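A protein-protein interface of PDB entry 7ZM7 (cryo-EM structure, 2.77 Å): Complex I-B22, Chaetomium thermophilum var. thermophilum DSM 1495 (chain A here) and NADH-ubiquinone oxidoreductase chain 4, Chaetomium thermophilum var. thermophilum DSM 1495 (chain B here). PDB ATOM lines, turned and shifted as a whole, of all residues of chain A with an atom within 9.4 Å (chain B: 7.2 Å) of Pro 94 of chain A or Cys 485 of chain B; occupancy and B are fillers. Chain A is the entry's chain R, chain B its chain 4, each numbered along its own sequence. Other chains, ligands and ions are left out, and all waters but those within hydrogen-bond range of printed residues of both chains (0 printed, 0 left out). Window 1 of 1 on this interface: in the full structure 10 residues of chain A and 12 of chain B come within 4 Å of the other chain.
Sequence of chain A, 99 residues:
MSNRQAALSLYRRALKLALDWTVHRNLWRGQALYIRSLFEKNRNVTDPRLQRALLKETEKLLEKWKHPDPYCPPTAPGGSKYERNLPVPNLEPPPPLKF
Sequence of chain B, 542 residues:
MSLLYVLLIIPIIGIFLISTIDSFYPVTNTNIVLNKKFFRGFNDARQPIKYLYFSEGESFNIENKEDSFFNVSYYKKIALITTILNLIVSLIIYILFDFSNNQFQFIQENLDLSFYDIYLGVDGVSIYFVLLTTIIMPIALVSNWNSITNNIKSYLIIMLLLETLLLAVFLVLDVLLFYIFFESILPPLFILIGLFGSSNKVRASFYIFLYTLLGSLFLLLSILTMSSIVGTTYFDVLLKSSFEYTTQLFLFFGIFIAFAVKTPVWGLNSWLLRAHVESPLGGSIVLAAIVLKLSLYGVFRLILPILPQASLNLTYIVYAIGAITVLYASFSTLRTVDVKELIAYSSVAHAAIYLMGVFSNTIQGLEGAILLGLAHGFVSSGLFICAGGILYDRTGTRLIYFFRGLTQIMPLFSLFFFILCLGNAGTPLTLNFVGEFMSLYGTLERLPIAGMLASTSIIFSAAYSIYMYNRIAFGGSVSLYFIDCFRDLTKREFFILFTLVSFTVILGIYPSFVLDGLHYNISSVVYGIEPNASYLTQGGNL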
ATOM      1  N   VAL A  88      23.840  20.870 -16.607  1.00  0.00           N
ATOM      2  CA  VAL A  88      22.818  19.930 -17.073  1.00  0.00           C
ATOM      3  C   VAL A  88      23.492  18.852 -17.912  1.00  0.00           C
ATOM      4  O   VAL A  88      24.382  19.163 -18.722  1.00  0.00           O
ATOM      5  CB  VAL A  88      21.729  20.670 -17.874  1.00  0.00           C
ATOM      6  CG1 VAL A  88      20.607  19.738 -18.243  1.00  0.00           C
ATOM      7  CG2 VAL A  88      21.190  21.844 -17.081  1.00  0.00           C
ATOM      8  N   PRO A  89      23.168  17.591 -17.732  1.00  0.00           N
ATOM      9  CA  PRO A  89      23.843  16.538 -18.496  1.00  0.00           C
ATOM     10  C   PRO A  89      23.286  16.351 -19.897  1.00  0.00           C
ATOM     11  O   PRO A  89      23.570  15.350 -20.552  1.00  0.00           O
ATOM     12  CB  PRO A  89      23.610  15.284 -17.641  1.00  0.00           C
ATOM     13  CG  PRO A  89      23.047  15.771 -16.341  1.00  0.00           C
ATOM     14  CD  PRO A  89      22.364  17.037 -16.633  1.00  0.00           C
ATOM     15  N   ASN A  90      22.491  17.300 -20.361  1.00  0.00           N
ATOM     16  CA  ASN A  90      21.794  17.187 -21.637  1.00  0.00           C
ATOM     17  C   ASN A  90      21.395  18.595 -22.046  1.00  0.00           C
ATOM     18  O   ASN A  90      20.439  19.146 -21.498  1.00  0.00           O
ATOM     19  CB  ASN A  90      20.572  16.283 -21.502  1.00  0.00           C
ATOM     20  CG  ASN A  90      19.893  15.995 -22.818  1.00  0.00           C
ATOM     21  OD1 ASN A  90      19.830  16.836 -23.699  1.00  0.00           O
ATOM     22  ND2 ASN A  90      19.339  14.806 -22.934  1.00  0.00           N
ATOM     23  N   LEU A  91      22.109  19.176 -23.000  1.00  0.00           N
ATOM     24  CA  LEU A  91      21.855  20.549 -23.396  1.00  0.00           C
ATOM     25  C   LEU A  91      21.120  20.664 -24.718  1.00  0.00           C
ATOM     26  O   LEU A  91      20.856  21.785 -25.163  1.00  0.00           O
ATOM     27  CB  LEU A  91      23.167  21.333 -23.497  1.00  0.00           C
ATOM     28  CG  LEU A  91      24.222  21.294 -22.403  1.00  0.00           C
ATOM     29  CD1 LEU A  91      25.323  22.238 -22.810  1.00  0.00           C
ATOM     30  CD2 LEU A  91      23.673  21.676 -21.046  1.00  0.00           C
ATOM     31  N   GLU A  92      20.816  19.555 -25.373  1.00  0.00           N
ATOM     32  CA  GLU A  92      20.078  19.631 -26.615  1.00  0.00           C
ATOM     33  C   GLU A  92      18.641  20.069 -26.349  1.00  0.00           C
ATOM     34  O   GLU A  92      18.067  19.749 -25.304  1.00  0.00           O
ATOM     35  CB  GLU A  92      20.091  18.288 -27.337  1.00  0.00           C
ATOM     36  CG  GLU A  92      21.443  17.906 -27.909  1.00  0.00           C
ATOM     37  CD  GLU A  92      22.374  17.278 -26.891  1.00  0.00           C
ATOM     38  OE1 GLU A  92      21.954  17.076 -25.733  1.00  0.00           O
ATOM     39  OE2 GLU A  92      23.533  16.984 -27.252  1.00  0.00           O
ATOM     40  N   PRO A  93      18.031  20.887 -27.249  1.00  0.00           N
ATOM     41  CA  PRO A  93      16.633  21.252 -27.107  1.00  0.00           C
ATOM     42  C   PRO A  93      15.819  19.958 -27.018  1.00  0.00           C
ATOM     43  O   PRO A  93      16.222  18.970 -27.593  1.00  0.00           O
ATOM     44  CB  PRO A  93      16.326  21.906 -28.450  1.00  0.00           C
ATOM     45  CG  PRO A  93      17.586  22.640 -28.768  1.00  0.00           C
ATOM     46  CD  PRO A  93      18.633  21.617 -28.396  1.00  0.00           C
ATOM     47  N   PRO A  94      14.652  19.962 -26.345  1.00  0.00           N
ATOM     48  CA  PRO A  94      13.871  18.744 -26.181  1.00  0.00           C
ATOM     49  C   PRO A  94      13.234  18.356 -27.526  1.00  0.00           C
ATOM     50  O   PRO A  94      13.080  19.218 -28.361  1.00  0.00           O
ATOM     51  CB  PRO A  94      12.830  19.159 -25.127  1.00  0.00           C
ATOM     52  CG  PRO A  94      13.266  20.508 -24.615  1.00  0.00           C
ATOM     53  CD  PRO A  94      14.004  21.133 -25.773  1.00  0.00           C
ATOM     54  N   PRO A  95      12.845  17.087 -27.772  1.00  0.00           N
ATOM     55  CA  PRO A  95      12.173  16.765 -29.036  1.00  0.00           C
ATOM     56  C   PRO A  95      10.731  17.301 -29.031  1.00  0.00           C
ATOM     57  O   PRO A  95      10.095  17.204 -28.009  1.00  0.00           O
ATOM     58  CB  PRO A  95      12.136  15.238 -29.039  1.00  0.00           C
ATOM     59  CG  PRO A  95      12.272  14.849 -27.586  1.00  0.00           C
ATOM     60  CD  PRO A  95      13.116  15.925 -26.936  1.00  0.00           C
ATOM     61  N   PRO A  96      10.168  17.849 -30.138  1.00  0.00           N
ATOM     62  CA  PRO A  96       8.872  18.538 -30.076  1.00  0.00           C
ATOM     63  C   PRO A  96       7.704  17.623 -29.736  1.00  0.00           C
ATOM     64  O   PRO A  96       7.270  16.820 -30.563  1.00  0.00           O
ATOM     65  CB  PRO A  96       8.724  19.120 -31.484  1.00  0.00           C
ATOM     66  CG  PRO A  96       9.581  18.284 -32.330  1.00  0.00           C
ATOM     67  CD  PRO A  96      10.740  17.880 -31.492  1.00  0.00           C
ATOM     68  N   LEU A  97       7.180  17.749 -28.523  1.00  0.00           N
ATOM     69  CA  LEU A  97       6.032  16.972 -28.086  1.00  0.00           C
ATOM     70  C   LEU A  97       5.023  17.882 -27.395  1.00  0.00           C
ATOM     71  O   LEU A  97       5.388  18.710 -26.560  1.00  0.00           O
ATOM     72  CB  LEU A  97       6.464  15.836 -27.152  1.00  0.00           C
ATOM     73  CG  LEU A  97       7.182  14.666 -27.815  1.00  0.00           C
ATOM     74  CD1 LEU A  97       7.680  13.727 -26.787  1.00  0.00           C
ATOM     75  CD2 LEU A  97       6.238  13.955 -28.756  1.00  0.00           C
ATOM     76  N   PHE A  99       1.773  18.995 -25.050  1.00  0.00           N
ATOM     77  CA  PHE A  99       1.291  18.642 -23.718  1.00  0.00           C
ATOM     78  C   PHE A  99       0.179  19.548 -23.209  1.00  0.00           C
ATOM     79  O   PHE A  99      -0.759  19.074 -22.568  1.00  0.00           O
ATOM     80  CB  PHE A  99       2.453  18.641 -22.723  1.00  0.00           C
ATOM     81  CG  PHE A  99       3.379  17.500 -22.916  1.00  0.00           C
ATOM     82  CD1 PHE A  99       2.906  16.209 -22.855  1.00  0.00           C
ATOM     83  CD2 PHE A  99       4.709  17.708 -23.212  1.00  0.00           C
ATOM     84  CE1 PHE A  99       3.747  15.151 -23.057  1.00  0.00           C
ATOM     85  CE2 PHE A  99       5.552  16.644 -23.409  1.00  0.00           C
ATOM     86  CZ  PHE A  99       5.072  15.367 -23.328  1.00  0.00           C
ATOM     87  N   GLN B 408      16.635  22.375 -13.008  1.00  0.00           N
ATOM     88  CA  GLN B 408      17.606  22.782 -14.007  1.00  0.00           C
ATOM     89  C   GLN B 408      16.991  22.979 -15.379  1.00  0.00           C
ATOM     90  O   GLN B 408      17.510  23.779 -16.159  1.00  0.00           O
ATOM     91  CB  GLN B 408      18.740  21.769 -14.070  1.00  0.00           C
ATOM     92  CG  GLN B 408      19.600  21.748 -12.822  1.00  0.00           C
ATOM     93  CD  GLN B 408      21.054  21.451 -13.120  1.00  0.00           C
ATOM     94  OE1 GLN B 408      21.460  20.297 -13.222  1.00  0.00           O
ATOM     95  NE2 GLN B 408      21.846  22.496 -13.268  1.00  0.00           N
ATOM     96  N   ILE B 409      15.896  22.295 -15.685  1.00  0.00           N
ATOM     97  CA  ILE B 409      15.278  22.397 -16.999  1.00  0.00           C
ATOM     98  C   ILE B 409      13.833  22.862 -16.949  1.00  0.00           C
ATOM     99  O   ILE B 409      13.279  23.203 -18.004  1.00  0.00           O
ATOM    100  CB  ILE B 409      15.385  21.064 -17.773  1.00  0.00           C
ATOM    101  CG1 ILE B 409      14.910  19.903 -16.902  1.00  0.00           C
ATOM    102  CG2 ILE B 409      16.799  20.859 -18.309  1.00  0.00           C
ATOM    103  CD1 ILE B 409      14.726  18.631 -17.633  1.00  0.00           C
ATOM    104  N   VAL B 478      19.798  17.051 -13.184  1.00  0.00           N
ATOM    105  CA  VAL B 478      18.808  16.416 -14.040  1.00  0.00           C
ATOM    106  C   VAL B 478      19.145  14.939 -14.157  1.00  0.00           C
ATOM    107  O   VAL B 478      20.286  14.566 -14.438  1.00  0.00           O
ATOM    108  CB  VAL B 478      18.748  17.105 -15.412  1.00  0.00           C
ATOM    109  CG1 VAL B 478      17.908  16.290 -16.346  1.00  0.00           C
ATOM    110  CG2 VAL B 478      18.159  18.471 -15.268  1.00  0.00           C
ATOM    111  N   PHE B 482      16.412  10.450 -17.810  1.00  0.00           N
ATOM    112  CA  PHE B 482      15.837  11.317 -18.831  1.00  0.00           C
ATOM    113  C   PHE B 482      16.765  11.279 -20.034  1.00  0.00           C
ATOM    114  O   PHE B 482      17.820  11.909 -20.033  1.00  0.00           O
ATOM    115  CB  PHE B 482      15.664  12.735 -18.300  1.00  0.00           C
ATOM    116  CG  PHE B 482      14.698  12.842 -17.157  1.00  0.00           C
ATOM    117  CD1 PHE B 482      13.887  11.776 -16.807  1.00  0.00           C
ATOM    118  CD2 PHE B 482      14.605  14.006 -16.422  1.00  0.00           C
ATOM    119  CE1 PHE B 482      13.000  11.873 -15.742  1.00  0.00           C
ATOM    120  CE2 PHE B 482      13.723  14.098 -15.355  1.00  0.00           C
ATOM    121  CZ  PHE B 482      12.921  13.036 -15.021  1.00  0.00           C
ATOM    122  N   ILE B 483      16.386  10.513 -21.054  1.00  0.00           N
ATOM    123  CA  ILE B 483      17.222  10.371 -22.241  1.00  0.00           C
ATOM    124  C   ILE B 483      17.272  11.668 -23.035  1.00  0.00           C
ATOM    125  O   ILE B 483      18.336  12.080 -23.507  1.00  0.00           O
ATOM    126  CB  ILE B 483      16.727   9.198 -23.098  1.00  0.00           C
ATOM    127  CG1 ILE B 483      16.782   7.929 -22.278  1.00  0.00           C
ATOM    128  CG2 ILE B 483      17.576   9.042 -24.315  1.00  0.00           C
ATOM    129  CD1 ILE B 483      18.178   7.621 -21.844  1.00  0.00           C
ATOM    130  N   ASP B 484      16.141  12.324 -23.203  1.00  0.00           N
ATOM    131  CA  ASP B 484      16.085  13.612 -23.871  1.00  0.00           C
ATOM    132  C   ASP B 484      15.579  14.678 -22.908  1.00  0.00           C
ATOM    133  O   ASP B 484      15.218  14.395 -21.765  1.00  0.00           O
ATOM    134  CB  ASP B 484      15.221  13.506 -25.129  1.00  0.00           C
ATOM    135  CG  ASP B 484      13.979  12.716 -24.889  1.00  0.00           C
ATOM    136  OD1 ASP B 484      13.799  12.289 -23.736  1.00  0.00           O
ATOM    137  OD2 ASP B 484      13.223  12.477 -25.847  1.00  0.00           O
ATOM    138  N   CYS B 485      15.633  15.929 -23.351  1.00  0.00           N
ATOM    139  CA  CYS B 485      15.251  17.032 -22.436  1.00  0.00           C
ATOM    140  C   CYS B 485      13.729  17.098 -22.299  1.00  0.00           C
ATOM    141  O   CYS B 485      13.020  16.511 -23.132  1.00  0.00           O
ATOM    142  CB  CYS B 485      15.817  18.369 -22.892  1.00  0.00           C
ATOM    143  SG  CYS B 485      16.117  19.504 -21.516  1.00  0.00           S
ATOM    144  N   PHE B 486      13.253  17.769 -21.258  1.00  0.00           N
ATOM    145  CA  PHE B 486      11.795  17.872 -21.029  1.00  0.00           C
ATOM    146  C   PHE B 486      11.450  19.345 -21.117  1.00  0.00           C
ATOM    147  O   PHE B 486      12.116  20.132 -20.447  1.00  0.00           O
ATOM    148  CB  PHE B 486      11.409  17.432 -19.618  1.00  0.00           C
ATOM    149  CG  PHE B 486      11.448  15.948 -19.383  1.00  0.00           C
ATOM    150  CD1 PHE B 486      11.757  15.073 -20.410  1.00  0.00           C
ATOM    151  CD2 PHE B 486      11.168  15.429 -18.133  1.00  0.00           C
ATOM    152  CE1 PHE B 486      11.796  13.707 -20.192  1.00  0.00           C
ATOM    153  CE2 PHE B 486      11.196  14.063 -17.922  1.00  0.00           C
ATOM    154  CZ  PHE B 486      11.511  13.206 -18.948  1.00  0.00           C
ATOM    155  N   ARG B 487      10.411  19.678 -21.871  1.00  0.00           N
ATOM    156  CA  ARG B 487       9.985  21.088 -21.952  1.00  0.00           C
ATOM    157  C   ARG B 487       9.465  21.532 -20.580  1.00  0.00           C
ATOM    158  O   ARG B 487       9.049  20.676 -19.786  1.00  0.00           O
ATOM    159  CB  ARG B 487       8.936  21.259 -23.056  1.00  0.00           C
ATOM    160  CG  ARG B 487       7.566  20.688 -22.727  1.00  0.00           C
ATOM    161  CD  ARG B 487       6.606  20.803 -23.893  1.00  0.00           C
ATOM    162  NE  ARG B 487       6.526  22.147 -24.441  1.00  0.00           N
ATOM    163  CZ  ARG B 487       5.742  22.497 -25.452  1.00  0.00           C
ATOM    164  NH1 ARG B 487       5.733  23.744 -25.884  1.00  0.00           N
ATOM    165  NH2 ARG B 487       4.961  21.600 -26.024  1.00  0.00           N
ATOM    166  N   ASP B 488       9.497  22.834 -20.319  1.00  0.00           N
ATOM    167  CA  ASP B 488       8.947  23.385 -19.058  1.00  0.00           C
ATOM    168  C   ASP B 488       7.436  23.540 -19.243  1.00  0.00           C
ATOM    169  O   ASP B 488       6.887  22.921 -20.165  1.00  0.00           O
ATOM    170  CB  ASP B 488       9.695  24.648 -18.625  1.00  0.00           C
ATOM    171  CG  ASP B 488       9.389  25.169 -17.231  1.00  0.00           C
ATOM    172  OD1 ASP B 488       8.662  24.490 -16.485  1.00  0.00           O
ATOM    173  OD2 ASP B 488       9.894  26.254 -16.899  1.00  0.00           O
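The side-chain amide nitrogen (ND2) of Asn 90 of chain A lies within hydrogen-bond range of the backbone carbonyl oxygen (O) of Ile 483 of chain B (3.0 Å).
O of Leu 97 of chain A sits at hydrogen-bond distance from NH2 of Arg 487 of chain B, at 3.0 Å.
The side-chain amide oxygen of Asn 90 of chain A sits close to the side-chain carboxylate of Glu 92 of chain A (3.0 Å).
Among the printed residues, merely in contact across the chains: Val 88 of chain A with Gln 408 of chain B (3.9 Å), Val 88 of chain A with Ile 409 of chain B (3.97 Å), Pro 89 of chain A with Val 478 of chain B (3.6 Å), Asn 90 of chain A with Asp 484 of chain B (3.6 Å), Asn 90 of chain A with Cys 485 of chain B (3.9 Å), Glu 92 of chain A with Cys 485 of chain B (3.6 Å), Pro 94 of chain A with Cys 485 of chain B (3.3 Å), Pro 95 of chain A with Asp 484 of chain B (3.1 Å), Pro 95 of chain A with Cys 485 of chain B (3.9 Å) and Phe 99 of chain A with Arg 487 of chain B (3.7 Å).
Leu 91 of chain A touches none of the printed residues of chain B.
Of the printed residues of chain B, Glu 92 of chain A touches Cys 485.
Pro 93 of chain A touches none of the printed residues of chain B.
Of the printed residues of chain A, Ile 483 of chain B touches Asn 90.
Asp 484 of chain B touches just these residues of chain A: Asn 90 (3.6 Å) and Pro 95 (3.1 Å).
Printed residues of chain A within 4 Å of Cys 485 of chain B: Asn 90 (3.9 Å), Glu 92 (3.6 Å), Pro 94 (3.3 Å) and Pro 95 (3.9 Å).
Of the printed residues of chain A, Arg 487 of chain B touches Leu 97 and Phe 99.
Printed residues of chain B that touch a printed residue of chain A: Gln 408, Ile 409, Val 478, Ile 483, Asp 484, Cys 485 and Arg 487.
Along chain B the printed residues that touch a printed residue of chain A span positions 408 to 487.
Printed residues of chain A that touch a printed residue of chain B: Val 88, Pro 89, Asn 90, Glu 92, Pro 94, Pro 95, Leu 97 and Phe 99.
Among the printed residues, no Asp or Glu carboxylate lies within 4 Å of a Lys or Arg side-chain nitrogen of the other chain.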
